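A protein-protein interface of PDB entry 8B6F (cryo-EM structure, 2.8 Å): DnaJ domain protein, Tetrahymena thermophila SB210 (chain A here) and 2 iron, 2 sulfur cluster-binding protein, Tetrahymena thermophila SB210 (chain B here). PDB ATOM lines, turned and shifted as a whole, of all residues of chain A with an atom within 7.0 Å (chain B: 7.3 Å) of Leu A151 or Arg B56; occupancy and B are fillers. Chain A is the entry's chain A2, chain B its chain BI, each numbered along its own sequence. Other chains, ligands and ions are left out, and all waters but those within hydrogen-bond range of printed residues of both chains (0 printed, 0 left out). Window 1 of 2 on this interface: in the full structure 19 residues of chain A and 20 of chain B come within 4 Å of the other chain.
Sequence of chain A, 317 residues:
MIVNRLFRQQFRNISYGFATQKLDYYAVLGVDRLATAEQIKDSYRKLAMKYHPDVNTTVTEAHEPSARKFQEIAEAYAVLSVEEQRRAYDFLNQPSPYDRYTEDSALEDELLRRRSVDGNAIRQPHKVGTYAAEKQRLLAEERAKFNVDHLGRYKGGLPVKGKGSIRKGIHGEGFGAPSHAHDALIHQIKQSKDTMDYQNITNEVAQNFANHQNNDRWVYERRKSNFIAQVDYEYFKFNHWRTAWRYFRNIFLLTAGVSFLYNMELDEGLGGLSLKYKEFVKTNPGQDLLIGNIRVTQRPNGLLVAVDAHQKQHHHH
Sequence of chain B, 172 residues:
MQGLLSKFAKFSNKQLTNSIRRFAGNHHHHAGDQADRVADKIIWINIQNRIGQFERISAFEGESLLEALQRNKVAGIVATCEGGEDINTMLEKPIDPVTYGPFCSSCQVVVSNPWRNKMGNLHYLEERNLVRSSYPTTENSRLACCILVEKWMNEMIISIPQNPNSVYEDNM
O of Gly A119 lies close to NE of Arg A115, at 3.4 Å.
The side-chain amide nitrogen (ND2) of Asn A120 sits at hydrogen-bond distance from the side-chain carboxylate (OD2) of Asp A118 (2.8 Å).
N of Leu A151 sits close to OD1 of Asp A149, 3.3 Å away.
The side-chain amide oxygen of Asn B154 lies within hydrogen-bond range of the backbone NH of Trp B44, 3.2 Å away.
O of Ile B47 is in hydrogen-bond range of N of Glu B55 (2.9 Å).
NH1 of Arg B56 lies within salt-bridge range of OE1 of Glu B155 (3.0 Å).
NH2 of Arg A115 touches CD1 of Trp B44 (3.8 Å).
Asp A118 touches Trp B44 (O to CZ2, 3.5 Å).
Trp B44 touches Asn A120 (CZ2 to OD1, 3.6 Å).
Leu A151 touches Trp B44.
Arg B56 touches Leu A151 (O to CD1, 3.8 Å).
Ala A181 touches Glu B55.
NH2 of Arg A115 sits close to ND2 of Asn B154 (3.2 Å).
The backbone carbonyl oxygen (O) of Gly A119 sits at hydrogen-bond distance from the indole nitrogen (NE1) of Trp B44 (3.0 Å).
OD1 of Asn A120 lies within hydrogen-bond range of NE of Arg B56 (3.4 Å).
NH1 of Arg A153 lies within salt-bridge range of OE1 of Glu B55, 2.8 Å away.
The guanidinium group (NH2) of Arg A153 sits at hydrogen-bond distance from the backbone carbonyl oxygen (O) of Asn B72, 2.7 Å away.
Hydrophobic or aromatic side chains of chain B within 4 Å of the printed part of chain A: Trp B44.
Hydrophobic or aromatic side chains of chain A within 4 Å of the printed part of chain B: Leu A151 and Ala A181.
Along chain A the printed residues that touch a printed residue of chain B span positions 115 to 181.
Among the printed residues, 11 pairs touch across the chains.
Among the printed residues, Asp or Glu carboxylates within 4 Å of a Lys or Arg side-chain nitrogen of the other chain: Arg A153 with Glu B55.
Printed residues of chain B within 4 Å of Arg A115: Trp B44 and Asn B154.
Leu A151 touches two residues of chain B.
Of the printed residues of chain B, Ala A181 touches Glu B55 (3.8 Å).
Ile B47 touches none of the printed residues of chain A.
Arg B56 touches just these residues of chain A: Asn A120 and Leu A151.
Of the printed residues of chain A, Asn B154 touches Arg A115 (3.2 Å).
The nearest residue of chain B that does not touch Leu A151 is Glu B55 (5.2 Å).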
ATOM      1  N   ARG A 115     -21.507  20.376  18.295  1.00  0.00           N
ATOM      2  CA  ARG A 115     -22.279  19.418  19.071  1.00  0.00           C
ATOM      3  C   ARG A 115     -23.764  19.539  18.753  1.00  0.00           C
ATOM      4  O   ARG A 115     -24.243  20.576  18.288  1.00  0.00           O
ATOM      5  CB  ARG A 115     -22.061  19.621  20.575  1.00  0.00           C
ATOM      6  CG  ARG A 115     -20.655  19.302  21.045  1.00  0.00           C
ATOM      7  CD  ARG A 115     -20.499  19.602  22.524  1.00  0.00           C
ATOM      8  NE  ARG A 115     -19.275  19.033  23.072  1.00  0.00           N
ATOM      9  CZ  ARG A 115     -18.948  19.058  24.356  1.00  0.00           C
ATOM     10  NH1 ARG A 115     -19.735  19.620  25.258  1.00  0.00           N
ATOM     11  NH2 ARG A 115     -17.806  18.502  24.746  1.00  0.00           N
ATOM     12  N   ASP A 118     -28.146  17.133  22.275  1.00  0.00           N
ATOM     13  CA  ASP A 118     -27.809  16.272  23.401  1.00  0.00           C
ATOM     14  C   ASP A 118     -26.389  16.489  23.904  1.00  0.00           C
ATOM     15  O   ASP A 118     -26.036  15.947  24.956  1.00  0.00           O
ATOM     16  CB  ASP A 118     -28.001  14.803  23.016  1.00  0.00           C
ATOM     17  CG  ASP A 118     -27.146  14.391  21.837  1.00  0.00           C
ATOM     18  OD1 ASP A 118     -26.369  15.231  21.341  1.00  0.00           O
ATOM     19  OD2 ASP A 118     -27.252  13.226  21.403  1.00  0.00           O
ATOM     20  N   GLY A 119     -25.571  17.258  23.188  1.00  0.00           N
ATOM     21  CA  GLY A 119     -24.204  17.514  23.584  1.00  0.00           C
ATOM     22  C   GLY A 119     -23.178  16.624  22.920  1.00  0.00           C
ATOM     23  O   GLY A 119     -21.982  16.925  22.997  1.00  0.00           O
ATOM     24  N   ASN A 120     -23.602  15.538  22.285  1.00  0.00           N
ATOM     25  CA  ASN A 120     -22.673  14.682  21.566  1.00  0.00           C
ATOM     26  C   ASN A 120     -22.225  15.352  20.273  1.00  0.00           C
ATOM     27  O   ASN A 120     -22.986  16.072  19.622  1.00  0.00           O
ATOM     28  CB  ASN A 120     -23.320  13.334  21.262  1.00  0.00           C
ATOM     29  CG  ASN A 120     -23.763  12.606  22.513  1.00  0.00           C
ATOM     30  OD1 ASN A 120     -23.049  12.578  23.515  1.00  0.00           O
ATOM     31  ND2 ASN A 120     -24.952  12.019  22.465  1.00  0.00           N
ATOM     32  N   ALA A 121     -20.972  15.109  19.903  1.00  0.00           N
ATOM     33  CA  ALA A 121     -20.429  15.681  18.682  1.00  0.00           C
ATOM     34  C   ALA A 121     -21.149  15.121  17.460  1.00  0.00           C
ATOM     35  O   ALA A 121     -21.665  14.000  17.472  1.00  0.00           O
ATOM     36  CB  ALA A 121     -18.931  15.399  18.579  1.00  0.00           C
ATOM     37  N   ARG A 123     -21.791  13.294  14.182  1.00  0.00           N
ATOM     38  CA  ARG A 123     -21.207  12.141  13.517  1.00  0.00           C
ATOM     39  C   ARG A 123     -22.060  11.761  12.316  1.00  0.00           C
ATOM     40  O   ARG A 123     -23.275  11.966  12.307  1.00  0.00           O
ATOM     41  CB  ARG A 123     -21.088  10.936  14.462  1.00  0.00           C
ATOM     42  CG  ARG A 123     -19.817  10.922  15.292  1.00  0.00           C
ATOM     43  CD  ARG A 123     -19.762   9.695  16.188  1.00  0.00           C
ATOM     44  NE  ARG A 123     -18.480   9.572  16.870  1.00  0.00           N
ATOM     45  CZ  ARG A 123     -18.147  10.229  17.974  1.00  0.00           C
ATOM     46  NH1 ARG A 123     -18.975  11.088  18.545  1.00  0.00           N
ATOM     47  NH2 ARG A 123     -16.952  10.019  18.517  1.00  0.00           N
ATOM     48  N   ARG A 143     -33.571  -0.628  24.085  1.00  0.00           N
ATOM     49  CA  ARG A 143     -33.477   0.367  25.148  1.00  0.00           C
ATOM     50  C   ARG A 143     -34.838   0.973  25.456  1.00  0.00           C
ATOM     51  O   ARG A 143     -35.169   1.221  26.621  1.00  0.00           O
ATOM     52  CB  ARG A 143     -32.477   1.456  24.764  1.00  0.00           C
ATOM     53  CG  ARG A 143     -31.036   0.980  24.723  1.00  0.00           C
ATOM     54  CD  ARG A 143     -30.071   2.152  24.695  1.00  0.00           C
ATOM     55  NE  ARG A 143     -30.385   3.088  23.622  1.00  0.00           N
ATOM     56  CZ  ARG A 143     -29.908   3.008  22.388  1.00  0.00           C
ATOM     57  NH1 ARG A 143     -29.081   2.040  22.027  1.00  0.00           N
ATOM     58  NH2 ARG A 143     -30.269   3.922  21.492  1.00  0.00           N
ATOM     59  N   VAL A 148     -34.440   2.778  28.901  1.00  0.00           N
ATOM     60  CA  VAL A 148     -33.053   3.212  28.996  1.00  0.00           C
ATOM     61  C   VAL A 148     -32.805   4.281  27.942  1.00  0.00           C
ATOM     62  O   VAL A 148     -33.253   4.152  26.799  1.00  0.00           O
ATOM     63  CB  VAL A 148     -32.078   2.029  28.816  1.00  0.00           C
ATOM     64  CG1 VAL A 148     -30.635   2.500  28.891  1.00  0.00           C
ATOM     65  CG2 VAL A 148     -32.347   0.968  29.861  1.00  0.00           C
ATOM     66  N   ASP A 149     -32.099   5.341  28.330  1.00  0.00           N
ATOM     67  CA  ASP A 149     -31.829   6.445  27.424  1.00  0.00           C
ATOM     68  C   ASP A 149     -30.726   6.059  26.441  1.00  0.00           C
ATOM     69  O   ASP A 149     -30.154   4.969  26.498  1.00  0.00           O
ATOM     70  CB  ASP A 149     -31.462   7.703  28.208  1.00  0.00           C
ATOM     71  CG  ASP A 149     -30.161   7.563  28.975  1.00  0.00           C
ATOM     72  OD1 ASP A 149     -29.554   6.473  28.936  1.00  0.00           O
ATOM     73  OD2 ASP A 149     -29.746   8.547  29.622  1.00  0.00           O
ATOM     74  N   HIS A 150     -30.417   6.975  25.521  1.00  0.00           N
ATOM     75  CA  HIS A 150     -29.465   6.674  24.459  1.00  0.00           C
ATOM     76  C   HIS A 150     -28.055   6.430  24.984  1.00  0.00           C
ATOM     77  O   HIS A 150     -27.253   5.803  24.285  1.00  0.00           O
ATOM     78  CB  HIS A 150     -29.448   7.811  23.434  1.00  0.00           C
ATOM     79  CG  HIS A 150     -29.016   9.128  23.996  1.00  0.00           C
ATOM     80  ND1 HIS A 150     -29.845   9.922  24.759  1.00  0.00           N
ATOM     81  CD2 HIS A 150     -27.843   9.796  23.898  1.00  0.00           C
ATOM     82  CE1 HIS A 150     -29.199  11.018  25.112  1.00  0.00           C
ATOM     83  NE2 HIS A 150     -27.982  10.967  24.602  1.00  0.00           N
ATOM     84  N   LEU A 151     -27.732   6.907  26.182  1.00  0.00           N
ATOM     85  CA  LEU A 151     -26.411   6.708  26.761  1.00  0.00           C
ATOM     86  C   LEU A 151     -26.330   5.476  27.651  1.00  0.00           C
ATOM     87  O   LEU A 151     -25.281   5.238  28.257  1.00  0.00           O
ATOM     88  CB  LEU A 151     -25.992   7.944  27.566  1.00  0.00           C
ATOM     89  CG  LEU A 151     -25.760   9.240  26.787  1.00  0.00           C
ATOM     90  CD1 LEU A 151     -25.299  10.338  27.727  1.00  0.00           C
ATOM     91  CD2 LEU A 151     -24.756   9.049  25.661  1.00  0.00           C
ATOM     92  N   GLY A 152     -27.402   4.696  27.755  1.00  0.00           N
ATOM     93  CA  GLY A 152     -27.370   3.484  28.541  1.00  0.00           C
ATOM     94  C   GLY A 152     -27.719   3.656  30.000  1.00  0.00           C
ATOM     95  O   GLY A 152     -27.233   2.886  30.836  1.00  0.00           O
ATOM     96  N   ARG A 153     -28.541   4.645  30.338  1.00  0.00           N
ATOM     97  CA  ARG A 153     -28.957   4.883  31.710  1.00  0.00           C
ATOM     98  C   ARG A 153     -30.470   5.026  31.757  1.00  0.00           C
ATOM     99  O   ARG A 153     -31.091   5.538  30.824  1.00  0.00           O
ATOM    100  CB  ARG A 153     -28.287   6.138  32.287  1.00  0.00           C
ATOM    101  CG  ARG A 153     -26.794   6.204  32.007  1.00  0.00           C
ATOM    102  CD  ARG A 153     -26.125   7.332  32.768  1.00  0.00           C
ATOM    103  NE  ARG A 153     -25.954   7.013  34.180  1.00  0.00           N
ATOM    104  CZ  ARG A 153     -24.957   6.294  34.674  1.00  0.00           C
ATOM    105  NH1 ARG A 153     -24.021   5.781  33.894  1.00  0.00           N
ATOM    106  NH2 ARG A 153     -24.893   6.087  35.986  1.00  0.00           N
ATOM    107  N   ALA A 181     -27.137   3.004  35.745  1.00  0.00           N
ATOM    108  CA  ALA A 181     -26.709   2.490  34.454  1.00  0.00           C
ATOM    109  C   ALA A 181     -27.341   1.136  34.165  1.00  0.00           C
ATOM    110  O   ALA A 181     -27.460   0.287  35.052  1.00  0.00           O
ATOM    111  CB  ALA A 181     -25.185   2.368  34.405  1.00  0.00           C
ATOM    112  N   HIS A 182     -27.744   0.945  32.914  1.00  0.00           N
ATOM    113  CA  HIS A 182     -28.340  -0.314  32.497  1.00  0.00           C
ATOM    114  C   HIS A 182     -27.284  -1.411  32.456  1.00  0.00           C
ATOM    115  O   HIS A 182     -26.127  -1.168  32.106  1.00  0.00           O
ATOM    116  CB  HIS A 182     -28.990  -0.153  31.125  1.00  0.00           C
ATOM    117  CG  HIS A 182     -29.771  -1.347  30.684  1.00  0.00           C
ATOM    118  ND1 HIS A 182     -30.636  -2.021  31.520  1.00  0.00           N
ATOM    119  CD2 HIS A 182     -29.823  -1.986  29.493  1.00  0.00           C
ATOM    120  CE1 HIS A 182     -31.185  -3.026  30.862  1.00  0.00           C
ATOM    121  NE2 HIS A 182     -30.707  -3.026  29.630  1.00  0.00           N
ATOM    122  N   ILE B  43     -18.832  18.586  29.876  1.00  0.00           N
ATOM    123  CA  ILE B  43     -17.595  17.872  29.584  1.00  0.00           C
ATOM    124  C   ILE B  43     -17.871  16.384  29.737  1.00  0.00           C
ATOM    125  O   ILE B  43     -18.352  15.939  30.786  1.00  0.00           O
ATOM    126  CB  ILE B  43     -16.462  18.327  30.520  1.00  0.00           C
ATOM    127  CG1 ILE B  43     -16.278  19.845  30.421  1.00  0.00           C
ATOM    128  CG2 ILE B  43     -15.169  17.614  30.171  1.00  0.00           C
ATOM    129  CD1 ILE B  43     -15.303  20.418  31.424  1.00  0.00           C
ATOM    130  N   TRP B  44     -17.558  15.614  28.700  1.00  0.00           N
ATOM    131  CA  TRP B  44     -17.928  14.207  28.648  1.00  0.00           C
ATOM    132  C   TRP B  44     -16.822  13.340  29.234  1.00  0.00           C
ATOM    133  O   TRP B  44     -15.652  13.476  28.867  1.00  0.00           O
ATOM    134  CB  TRP B  44     -18.229  13.785  27.211  1.00  0.00           C
ATOM    135  CG  TRP B  44     -19.500  14.366  26.686  1.00  0.00           C
ATOM    136  CD1 TRP B  44     -19.627  15.343  25.746  1.00  0.00           C
ATOM    137  CD2 TRP B  44     -20.828  14.008  27.078  1.00  0.00           C
ATOM    138  NE1 TRP B  44     -20.955  15.613  25.524  1.00  0.00           N
ATOM    139  CE2 TRP B  44     -21.712  14.808  26.332  1.00  0.00           C
ATOM    140  CE3 TRP B  44     -21.355  13.088  27.989  1.00  0.00           C
ATOM    141  CZ2 TRP B  44     -23.093  14.711  26.463  1.00  0.00           C
ATOM    142  CZ3 TRP B  44     -22.724  12.995  28.121  1.00  0.00           C
ATOM    143  CH2 TRP B  44     -23.579  13.802  27.362  1.00  0.00           C
ATOM    144  N   ILE B  45     -17.206  12.443  30.138  1.00  0.00           N
ATOM    145  CA  ILE B  45     -16.296  11.505  30.782  1.00  0.00           C
ATOM    146  C   ILE B  45     -16.734  10.098  30.410  1.00  0.00           C
ATOM    147  O   ILE B  45     -17.892   9.725  30.628  1.00  0.00           O
ATOM    148  CB  ILE B  45     -16.279  11.687  32.311  1.00  0.00           C
ATOM    149  CG1 ILE B  45     -15.886  13.121  32.682  1.00  0.00           C
ATOM    150  CG2 ILE B  45     -15.335  10.684  32.961  1.00  0.00           C
ATOM    151  CD1 ILE B  45     -14.500  13.532  32.224  1.00  0.00           C
ATOM    152  N   ASN B  46     -15.809   9.320  29.859  1.00  0.00           N
ATOM    153  CA  ASN B  46     -16.068   7.940  29.474  1.00  0.00           C
ATOM    154  C   ASN B  46     -15.454   7.015  30.516  1.00  0.00           C
ATOM    155  O   ASN B  46     -14.305   7.207  30.922  1.00  0.00           O
ATOM    156  CB  ASN B  46     -15.492   7.648  28.089  1.00  0.00           C
ATOM    157  CG  ASN B  46     -16.013   8.600  27.035  1.00  0.00           C
ATOM    158  OD1 ASN B  46     -17.209   8.873  26.968  1.00  0.00           O
ATOM    159  ND2 ASN B  46     -15.116   9.121  26.213  1.00  0.00           N
ATOM    160  N   ILE B  47     -16.222   6.016  30.940  1.00  0.00           N
ATOM    161  CA  ILE B  47     -15.872   5.174  32.074  1.00  0.00           C
ATOM    162  C   ILE B  47     -16.022   3.713  31.680  1.00  0.00           C
ATOM    163  O   ILE B  47     -16.940   3.350  30.938  1.00  0.00           O
ATOM    164  CB  ILE B  47     -16.755   5.489  33.299  1.00  0.00           C
ATOM    165  CG1 ILE B  47     -16.648   6.972  33.662  1.00  0.00           C
ATOM    166  CG2 ILE B  47     -16.349   4.621  34.478  1.00  0.00           C
ATOM    167  CD1 ILE B  47     -17.650   7.426  34.701  1.00  0.00           C
ATOM    168  N   PHE B  54     -19.357  -0.090  29.421  1.00  0.00           N
ATOM    169  CA  PHE B  54     -18.952   1.276  29.127  1.00  0.00           C
ATOM    170  C   PHE B  54     -20.062   2.250  29.493  1.00  0.00           C
ATOM    171  O   PHE B  54     -21.242   1.981  29.252  1.00  0.00           O
ATOM    172  CB  PHE B  54     -18.596   1.433  27.647  1.00  0.00           C
ATOM    173  CG  PHE B  54     -17.501   0.518  27.190  1.00  0.00           C
ATOM    174  CD1 PHE B  54     -16.243   0.590  27.756  1.00  0.00           C
ATOM    175  CD2 PHE B  54     -17.727  -0.407  26.188  1.00  0.00           C
ATOM    176  CE1 PHE B  54     -15.232  -0.250  27.340  1.00  0.00           C
ATOM    177  CE2 PHE B  54     -16.720  -1.249  25.765  1.00  0.00           C
ATOM    178  CZ  PHE B  54     -15.470  -1.169  26.342  1.00  0.00           C
ATOM    179  N   GLU B  55     -19.674   3.382  30.074  1.00  0.00           N
ATOM    180  CA  GLU B  55     -20.606   4.421  30.470  1.00  0.00           C
ATOM    181  C   GLU B  55     -20.084   5.773  30.010  1.00  0.00           C
ATOM    182  O   GLU B  55     -18.877   5.969  29.854  1.00  0.00           O
ATOM    183  CB  GLU B  55     -20.814   4.439  31.988  1.00  0.00           C
ATOM    184  CG  GLU B  55     -21.140   3.079  32.579  1.00  0.00           C
ATOM    185  CD  GLU B  55     -21.461   3.150  34.057  1.00  0.00           C
ATOM    186  OE1 GLU B  55     -21.782   4.254  34.543  1.00  0.00           O
ATOM    187  OE2 GLU B  55     -21.390   2.103  34.734  1.00  0.00           O
ATOM    188  N   ARG B  56     -21.008   6.706  29.803  1.00  0.00           N
ATOM    189  CA  ARG B  56     -20.672   8.054  29.364  1.00  0.00           C
ATOM    190  C   ARG B  56     -21.495   9.034  30.182  1.00  0.00           C
ATOM    191  O   ARG B  56     -22.727   8.968  30.170  1.00  0.00           O
ATOM    192  CB  ARG B  56     -20.950   8.224  27.868  1.00  0.00           C
ATOM    193  CG  ARG B  56     -20.582   9.581  27.295  1.00  0.00           C
ATOM    194  CD  ARG B  56     -20.888   9.619  25.808  1.00  0.00           C
ATOM    195  NE  ARG B  56     -20.619  10.920  25.207  1.00  0.00           N
ATOM    196  CZ  ARG B  56     -19.433  11.313  24.765  1.00  0.00           C
ATOM    197  NH1 ARG B  56     -18.364  10.544  24.878  1.00  0.00           N
ATOM    198  NH2 ARG B  56     -19.317  12.508  24.196  1.00  0.00           N
ATOM    199  N   ILE B  57     -20.820   9.934  30.894  1.00  0.00           N
ATOM    200  CA  ILE B  57     -21.474  10.870  31.794  1.00  0.00           C
ATOM    201  C   ILE B  57     -20.996  12.277  31.468  1.00  0.00           C
ATOM    202  O   ILE B  57     -20.026  12.477  30.736  1.00  0.00           O
ATOM    203  CB  ILE B  57     -21.213  10.543  33.277  1.00  0.00           C
ATOM    204  CG1 ILE B  57     -19.720  10.657  33.587  1.00  0.00           C
ATOM    205  CG2 ILE B  57     -21.736   9.150  33.598  1.00  0.00           C
ATOM    206  CD1 ILE B  57     -19.390  10.469  35.033  1.00  0.00           C
ATOM    207  N   SER B  58     -21.694  13.255  32.032  1.00  0.00           N
ATOM    208  CA  SER B  58     -21.411  14.665  31.816  1.00  0.00           C
ATOM    209  C   SER B  58     -21.010  15.318  33.128  1.00  0.00           C
ATOM    210  O   SER B  58     -21.583  15.024  34.181  1.00  0.00           O
ATOM    211  CB  SER B  58     -22.619  15.386  31.227  1.00  0.00           C
ATOM    212  OG  SER B  58     -23.738  15.272  32.083  1.00  0.00           O
ATOM    213  N   ASN B  72     -24.142  11.527  38.682  1.00  0.00           N
ATOM    214  CA  ASN B  72     -24.566  10.587  37.654  1.00  0.00           C
ATOM    215  C   ASN B  72     -24.781   9.181  38.193  1.00  0.00           C
ATOM    216  O   ASN B  72     -25.222   8.306  37.440  1.00  0.00           O
ATOM    217  CB  ASN B  72     -23.535  10.556  36.524  1.00  0.00           C
ATOM    218  CG  ASN B  72     -23.513  11.843  35.728  1.00  0.00           C
ATOM    219  OD1 ASN B  72     -24.114  11.934  34.658  1.00  0.00           O
ATOM    220  ND2 ASN B  72     -22.825  12.850  36.251  1.00  0.00           N
ATOM    221  N   VAL B  74     -22.637   6.736  39.309  1.00  0.00           N
ATOM    222  CA  VAL B  74     -21.749   5.719  38.757  1.00  0.00           C
ATOM    223  C   VAL B  74     -21.378   4.741  39.862  1.00  0.00           C
ATOM    224  O   VAL B  74     -20.941   5.142  40.946  1.00  0.00           O
ATOM    225  CB  VAL B  74     -20.500   6.366  38.138  1.00  0.00           C
ATOM    226  CG1 VAL B  74     -19.472   5.309  37.749  1.00  0.00           C
ATOM    227  CG2 VAL B  74     -20.885   7.198  36.931  1.00  0.00           C
ATOM    228  N   ASN B 154     -12.076  16.811  28.390  1.00  0.00           N
ATOM    229  CA  ASN B 154     -13.182  16.361  27.557  1.00  0.00           C
ATOM    230  C   ASN B 154     -12.842  15.028  26.903  1.00  0.00           C
ATOM    231  O   ASN B 154     -11.745  14.847  26.370  1.00  0.00           O
ATOM    232  CB  ASN B 154     -13.495  17.411  26.493  1.00  0.00           C
ATOM    233  CG  ASN B 154     -14.783  17.125  25.754  1.00  0.00           C
ATOM    234  OD1 ASN B 154     -15.735  16.603  26.328  1.00  0.00           O
ATOM    235  ND2 ASN B 154     -14.817  17.464  24.472  1.00  0.00           N
ATOM    236  N   GLU B 155     -13.792  14.095  26.945  1.00  0.00           N
ATOM    237  CA  GLU B 155     -13.639  12.757  26.386  1.00  0.00           C
ATOM    238  C   GLU B 155     -12.606  11.923  27.132  1.00  0.00           C
ATOM    239  O   GLU B 155     -12.086  10.948  26.583  1.00  0.00           O
ATOM    240  CB  GLU B 155     -13.271  12.819  24.899  1.00  0.00           C
ATOM    241  CG  GLU B 155     -14.176  13.718  24.073  1.00  0.00           C
ATOM    242  CD  GLU B 155     -15.611  13.236  24.044  1.00  0.00           C
ATOM    243  OE1 GLU B 155     -15.855  12.066  24.406  1.00  0.00           O
ATOM    244  OE2 GLU B 155     -16.498  14.026  23.662  1.00  0.00           O
ATOM    245  N   MET B 156     -12.293  12.280  28.373  1.00  0.00           N
ATOM    246  CA  MET B 156     -11.315  11.528  29.144  1.00  0.00           C
ATOM    247  C   MET B 156     -11.838  10.135  29.472  1.00  0.00           C
ATOM    248  O   MET B 156     -12.990   9.966  29.879  1.00  0.00           O
ATOM    249  CB  MET B 156     -10.970  12.272  30.433  1.00  0.00           C
ATOM    250  CG  MET B 156      -9.982  11.533  31.323  1.00  0.00           C
ATOM    251  SD  MET B 156      -9.423  12.514  32.729  1.00  0.00           S
ATOM    252  CE  MET B 156     -10.960  12.762  33.615  1.00  0.00           C
